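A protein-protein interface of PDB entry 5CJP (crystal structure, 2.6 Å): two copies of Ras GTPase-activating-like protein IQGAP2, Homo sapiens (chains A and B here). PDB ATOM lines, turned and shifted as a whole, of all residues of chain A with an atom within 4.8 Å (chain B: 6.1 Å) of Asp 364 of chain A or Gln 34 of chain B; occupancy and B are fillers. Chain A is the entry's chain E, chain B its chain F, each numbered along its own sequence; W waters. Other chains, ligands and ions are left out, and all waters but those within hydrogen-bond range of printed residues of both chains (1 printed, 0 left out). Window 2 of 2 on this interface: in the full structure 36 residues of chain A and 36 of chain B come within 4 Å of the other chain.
OE1 of Gln 34 of chain B lies close to OD1 of Asp 364 of chain A, at 3.3 Å.
OG of Ser 367 of chain A sits at hydrogen-bond distance from O of Leu 31 of chain B, at 3.3 Å.
The backbone carbonyl oxygen (O) of Asn 363 of chain A sits at hydrogen-bond distance from the side-chain hydroxyl (OG) of Ser 367 of chain A (3.0 Å).
Among the printed residues, merely in contact across the chains: Asn 363 of chain A with Lys 30 of chain B (3.7 Å), Asn 363 of chain A with Leu 31 of chain B (3.6 Å), Asn 363 of chain A with Gln 34 of chain B (3.4 Å) and Ser 367 of chain A with Gln 34 of chain B (3.5 Å).
Asp 364 of chain A touches just one residue of chain B: Gln 34.
Of the printed residues of chain B, Ser 367 of chain A touches Leu 31 (3.3 Å) and Gln 34 (3.5 Å).
Of the printed residues of chain A, Lys 30 of chain B touches Asn 363.
Of the printed residues of chain A, Leu 31 of chain B touches Asn 363 and Ser 367.
Phe 33 of chain B touches none of the printed residues of chain A.
Gln 34 of chain B touches just these residues of chain A: Asn 363 (3.4 Å), Asp 364 (3.3 Å) and Ser 367 (3.5 Å).
Pro 36 of chain B touches none of the printed residues of chain A.
The nearest printed residue of chain A that does not touch Gln 34 of chain B is Pro 360 of chain A (6.1 Å).
Hydrophobic or aromatic side chains of chain B that line the printed part of chain A: Leu 31.
Of the 9 printed residues of chain A, 3 touch a printed residue of chain B.
Among the printed residues, no Asp or Glu carboxylate lies within 4 Å of a Lys or Arg side-chain nitrogen of the other chain.
No position is printed for both chains.
Of the 6 pairs that touch across the chains among the printed residues, none has its exchanged pair printed and touching as well.
Water W1 lies within hydrogen-bond range of the side-chain amide oxygen of Asn 363 of chain A and the side-chain amino group of Lys 30 of chain B.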
ATOM      1  N   PRO A 360     -14.887  26.328   2.276  1.00  0.00           N
ATOM      2  CA  PRO A 360     -13.597  26.891   1.851  1.00  0.00           C
ATOM      3  C   PRO A 360     -12.892  26.110   0.737  1.00  0.00           C
ATOM      4  O   PRO A 360     -12.370  25.009   0.962  1.00  0.00           O
ATOM      5  CB  PRO A 360     -12.774  26.892   3.140  1.00  0.00           C
ATOM      6  CG  PRO A 360     -13.804  26.922   4.220  1.00  0.00           C
ATOM      7  CD  PRO A 360     -14.840  25.963   3.702  1.00  0.00           C
ATOM      8  N   GLU A 361     -12.876  26.696  -0.457  1.00  0.00           N
ATOM      9  CA  GLU A 361     -12.230  26.072  -1.605  1.00  0.00           C
ATOM     10  C   GLU A 361     -10.710  26.117  -1.416  1.00  0.00           C
ATOM     11  O   GLU A 361      -9.965  25.425  -2.102  1.00  0.00           O
ATOM     12  CB  GLU A 361     -12.641  26.795  -2.897  1.00  0.00           C
ATOM     13  CG  GLU A 361     -12.181  28.249  -2.999  1.00  0.00           C
ATOM     14  CD  GLU A 361     -12.825  28.993  -4.166  1.00  0.00           C
ATOM     15  OE1 GLU A 361     -12.820  28.460  -5.299  1.00  0.00           O
ATOM     16  OE2 GLU A 361     -13.335  30.117  -3.948  1.00  0.00           O
ATOM     17  N   LYS A 362     -10.270  26.935  -0.469  1.00  0.00           N
ATOM     18  CA  LYS A 362      -8.856  27.085  -0.146  1.00  0.00           C
ATOM     19  C   LYS A 362      -8.316  25.843   0.592  1.00  0.00           C
ATOM     20  O   LYS A 362      -7.214  25.370   0.317  1.00  0.00           O
ATOM     21  CB  LYS A 362      -8.667  28.324   0.738  1.00  0.00           C
ATOM     22  CG  LYS A 362      -7.256  28.500   1.248  1.00  0.00           C
ATOM     23  CD  LYS A 362      -7.143  29.678   2.200  1.00  0.00           C
ATOM     24  CE  LYS A 362      -5.771  29.678   2.874  1.00  0.00           C
ATOM     25  NZ  LYS A 362      -5.621  30.750   3.897  1.00  0.00           N
ATOM     26  N   ASN A 363      -9.102  25.326   1.531  1.00  0.00           N
ATOM     27  CA  ASN A 363      -8.710  24.165   2.311  1.00  0.00           C
ATOM     28  C   ASN A 363      -8.571  22.941   1.431  1.00  0.00           C
ATOM     29  O   ASN A 363      -7.771  22.045   1.716  1.00  0.00           O
ATOM     30  CB  ASN A 363      -9.734  23.886   3.410  1.00  0.00           C
ATOM     31  CG  ASN A 363      -9.926  25.066   4.340  1.00  0.00           C
ATOM     32  OD1 ASN A 363     -10.646  24.970   5.328  1.00  0.00           O
ATOM     33  ND2 ASN A 363      -9.293  26.186   4.032  1.00  0.00           N
ATOM     34  N   ASP A 364      -9.348  22.895   0.362  1.00  0.00           N
ATOM     35  CA  ASP A 364      -9.292  21.753  -0.532  1.00  0.00           C
ATOM     36  C   ASP A 364      -8.084  21.856  -1.451  1.00  0.00           C
ATOM     37  O   ASP A 364      -7.339  20.890  -1.619  1.00  0.00           O
ATOM     38  CB  ASP A 364     -10.592  21.661  -1.325  1.00  0.00           C
ATOM     39  CG  ASP A 364     -11.811  21.575  -0.414  1.00  0.00           C
ATOM     40  OD1 ASP A 364     -11.792  20.759   0.537  1.00  0.00           O
ATOM     41  OD2 ASP A 364     -12.787  22.321  -0.649  1.00  0.00           O
ATOM     42  N   LEU A 365      -7.876  23.035  -2.023  1.00  0.00           N
ATOM     43  CA  LEU A 365      -6.732  23.231  -2.900  1.00  0.00           C
ATOM     44  C   LEU A 365      -5.452  22.983  -2.104  1.00  0.00           C
ATOM     45  O   LEU A 365      -4.603  22.194  -2.508  1.00  0.00           O
ATOM     46  CB  LEU A 365      -6.725  24.655  -3.468  1.00  0.00           C
ATOM     47  CG  LEU A 365      -7.839  24.998  -4.461  1.00  0.00           C
ATOM     48  CD1 LEU A 365      -7.643  26.414  -4.981  1.00  0.00           C
ATOM     49  CD2 LEU A 365      -7.826  24.003  -5.616  1.00  0.00           C
ATOM     50  N   LEU A 366      -5.341  23.653  -0.963  1.00  0.00           N
ATOM     51  CA  LEU A 366      -4.182  23.534  -0.109  1.00  0.00           C
ATOM     52  C   LEU A 366      -3.939  22.105   0.369  1.00  0.00           C
ATOM     53  O   LEU A 366      -2.789  21.714   0.595  1.00  0.00           O
ATOM     54  CB  LEU A 366      -4.331  24.498   1.078  1.00  0.00           C
ATOM     55  CG  LEU A 366      -3.264  25.597   1.289  1.00  0.00           C
ATOM     56  CD1 LEU A 366      -2.656  26.029  -0.048  1.00  0.00           C
ATOM     57  CD2 LEU A 366      -3.880  26.787   2.001  1.00  0.00           C
ATOM     58  N   SER A 367      -5.003  21.312   0.509  1.00  0.00           N
ATOM     59  CA  SER A 367      -4.865  19.931   0.962  1.00  0.00           C
ATOM     60  C   SER A 367      -4.429  19.012  -0.153  1.00  0.00           C
ATOM     61  O   SER A 367      -3.668  18.070   0.072  1.00  0.00           O
ATOM     62  CB  SER A 367      -6.176  19.406   1.549  1.00  0.00           C
ATOM     63  OG  SER A 367      -6.265  19.693   2.932  1.00  0.00           O
ATOM     64  N   GLU A 368      -4.935  19.267  -1.351  1.00  0.00           N
ATOM     65  CA  GLU A 368      -4.554  18.462  -2.506  1.00  0.00           C
ATOM     66  C   GLU A 368      -3.075  18.740  -2.773  1.00  0.00           C
ATOM     67  O   GLU A 368      -2.269  17.825  -2.944  1.00  0.00           O
ATOM     68  CB  GLU A 368      -5.369  18.867  -3.742  1.00  0.00           C
ATOM     69  CG  GLU A 368      -6.872  18.664  -3.622  1.00  0.00           C
ATOM     70  CD  GLU A 368      -7.255  17.210  -3.416  1.00  0.00           C
ATOM     71  OE1 GLU A 368      -6.874  16.367  -4.255  1.00  0.00           O
ATOM     72  OE2 GLU A 368      -7.939  16.913  -2.414  1.00  0.00           O
ATOM     73  N   ALA B  29      -2.258  21.591  10.647  1.00  0.00           N
ATOM     74  CA  ALA B  29      -2.801  20.405  11.303  1.00  0.00           C
ATOM     75  C   ALA B  29      -4.188  20.131  10.742  1.00  0.00           C
ATOM     76  O   ALA B  29      -4.484  19.018  10.314  1.00  0.00           O
ATOM     77  CB  ALA B  29      -2.894  20.639  12.798  1.00  0.00           C
ATOM     78  N   LYS B  30      -5.042  21.150  10.747  1.00  0.00           N
ATOM     79  CA  LYS B  30      -6.377  20.963  10.196  1.00  0.00           C
ATOM     80  C   LYS B  30      -6.336  20.416   8.761  1.00  0.00           C
ATOM     81  O   LYS B  30      -7.084  19.502   8.427  1.00  0.00           O
ATOM     82  CB  LYS B  30      -7.184  22.263  10.202  1.00  0.00           C
ATOM     83  CG  LYS B  30      -8.500  22.078   9.478  1.00  0.00           C
ATOM     84  CD  LYS B  30      -9.334  23.315   9.461  1.00  0.00           C
ATOM     85  CE  LYS B  30     -10.705  22.995   8.895  1.00  0.00           C
ATOM     86  NZ  LYS B  30     -11.548  24.224   8.813  1.00  0.00           N
ATOM     87  N   LEU B  31      -5.486  20.982   7.907  1.00  0.00           N
ATOM     88  CA  LEU B  31      -5.388  20.485   6.528  1.00  0.00           C
ATOM     89  C   LEU B  31      -4.920  19.027   6.516  1.00  0.00           C
ATOM     90  O   LEU B  31      -5.386  18.228   5.711  1.00  0.00           O
ATOM     91  CB  LEU B  31      -4.430  21.361   5.707  1.00  0.00           C
ATOM     92  CG  LEU B  31      -4.860  22.825   5.591  1.00  0.00           C
ATOM     93  CD1 LEU B  31      -3.719  23.609   4.941  1.00  0.00           C
ATOM     94  CD2 LEU B  31      -6.195  22.966   4.795  1.00  0.00           C
ATOM     95  N   ILE B  32      -3.990  18.697   7.415  1.00  0.00           N
ATOM     96  CA  ILE B  32      -3.488  17.323   7.535  1.00  0.00           C
ATOM     97  C   ILE B  32      -4.656  16.359   7.838  1.00  0.00           C
ATOM     98  O   ILE B  32      -4.732  15.256   7.269  1.00  0.00           O
ATOM     99  CB  ILE B  32      -2.437  17.186   8.689  1.00  0.00           C
ATOM    100  CG1 ILE B  32      -1.200  18.053   8.402  1.00  0.00           C
ATOM    101  CG2 ILE B  32      -2.023  15.760   8.866  1.00  0.00           C
ATOM    102  CD1 ILE B  32      -0.594  17.805   7.071  1.00  0.00           C
ATOM    103  N   PHE B  33      -5.568  16.767   8.727  1.00  0.00           N
ATOM    104  CA  PHE B  33      -6.713  15.912   9.074  1.00  0.00           C
ATOM    105  C   PHE B  33      -7.632  15.602   7.899  1.00  0.00           C
ATOM    106  O   PHE B  33      -8.083  14.458   7.763  1.00  0.00           O
ATOM    107  CB  PHE B  33      -7.575  16.513  10.204  1.00  0.00           C
ATOM    108  CG  PHE B  33      -6.829  16.771  11.481  1.00  0.00           C
ATOM    109  CD1 PHE B  33      -5.817  15.906  11.904  1.00  0.00           C
ATOM    110  CD2 PHE B  33      -7.117  17.901  12.251  1.00  0.00           C
ATOM    111  CE1 PHE B  33      -5.094  16.166  13.074  1.00  0.00           C
ATOM    112  CE2 PHE B  33      -6.401  18.168  13.422  1.00  0.00           C
ATOM    113  CZ  PHE B  33      -5.386  17.298  13.831  1.00  0.00           C
ATOM    114  N   GLN B  34      -7.912  16.592   7.049  1.00  0.00           N
ATOM    115  CA  GLN B  34      -8.815  16.332   5.929  1.00  0.00           C
ATOM    116  C   GLN B  34      -8.213  15.709   4.676  1.00  0.00           C
ATOM    117  O   GLN B  34      -8.947  15.429   3.728  1.00  0.00           O
ATOM    118  CB  GLN B  34      -9.644  17.577   5.544  1.00  0.00           C
ATOM    119  CG  GLN B  34      -8.888  18.790   5.050  1.00  0.00           C
ATOM    120  CD  GLN B  34      -9.795  19.765   4.280  1.00  0.00           C
ATOM    121  OE1 GLN B  34     -10.148  19.519   3.119  1.00  0.00           O
ATOM    122  NE2 GLN B  34     -10.183  20.862   4.930  1.00  0.00           N
ATOM    123  N   MET B  35      -6.899  15.476   4.667  1.00  0.00           N
ATOM    124  CA  MET B  35      -6.248  14.839   3.519  1.00  0.00           C
ATOM    125  C   MET B  35      -6.584  13.349   3.516  1.00  0.00           C
ATOM    126  O   MET B  35      -6.993  12.797   4.541  1.00  0.00           O
ATOM    127  CB  MET B  35      -4.723  14.944   3.610  1.00  0.00           C
ATOM    128  CG  MET B  35      -4.146  16.341   3.656  1.00  0.00           C
ATOM    129  SD  MET B  35      -2.316  16.339   3.687  1.00  0.00           S
ATOM    130  CE  MET B  35      -1.994  14.660   3.436  1.00  0.00           C
ATOM    131  N   PRO B  36      -6.434  12.680   2.360  1.00  0.00           N
ATOM    132  CA  PRO B  36      -6.735  11.248   2.367  1.00  0.00           C
ATOM    133  C   PRO B  36      -5.745  10.715   3.394  1.00  0.00           C
ATOM    134  O   PRO B  36      -4.607  11.190   3.451  1.00  0.00           O
ATOM    135  CB  PRO B  36      -6.384  10.809   0.948  1.00  0.00           C
ATOM    136  CG  PRO B  36      -6.642  12.032   0.140  1.00  0.00           C
ATOM    137  CD  PRO B  36      -6.085  13.144   1.007  1.00  0.00           C
ATOM    138  N   THR B  92      -7.096  10.400  11.544  1.00  0.00           N
ATOM    139  CA  THR B  92      -5.756  10.940  11.686  1.00  0.00           C
ATOM    140  C   THR B  92      -5.641  11.877  12.887  1.00  0.00           C
ATOM    141  O   THR B  92      -4.541  12.117  13.388  1.00  0.00           O
ATOM    142  CB  THR B  92      -5.213  11.595  10.343  1.00  0.00           C
ATOM    143  OG1 THR B  92      -4.873  12.972  10.554  1.00  0.00           O
ATOM    144  CG2 THR B  92      -6.215  11.465   9.224  1.00  0.00           C
HETATM  145  O   HOH W   1     -11.578  26.863   7.187  1.00  0.00           O
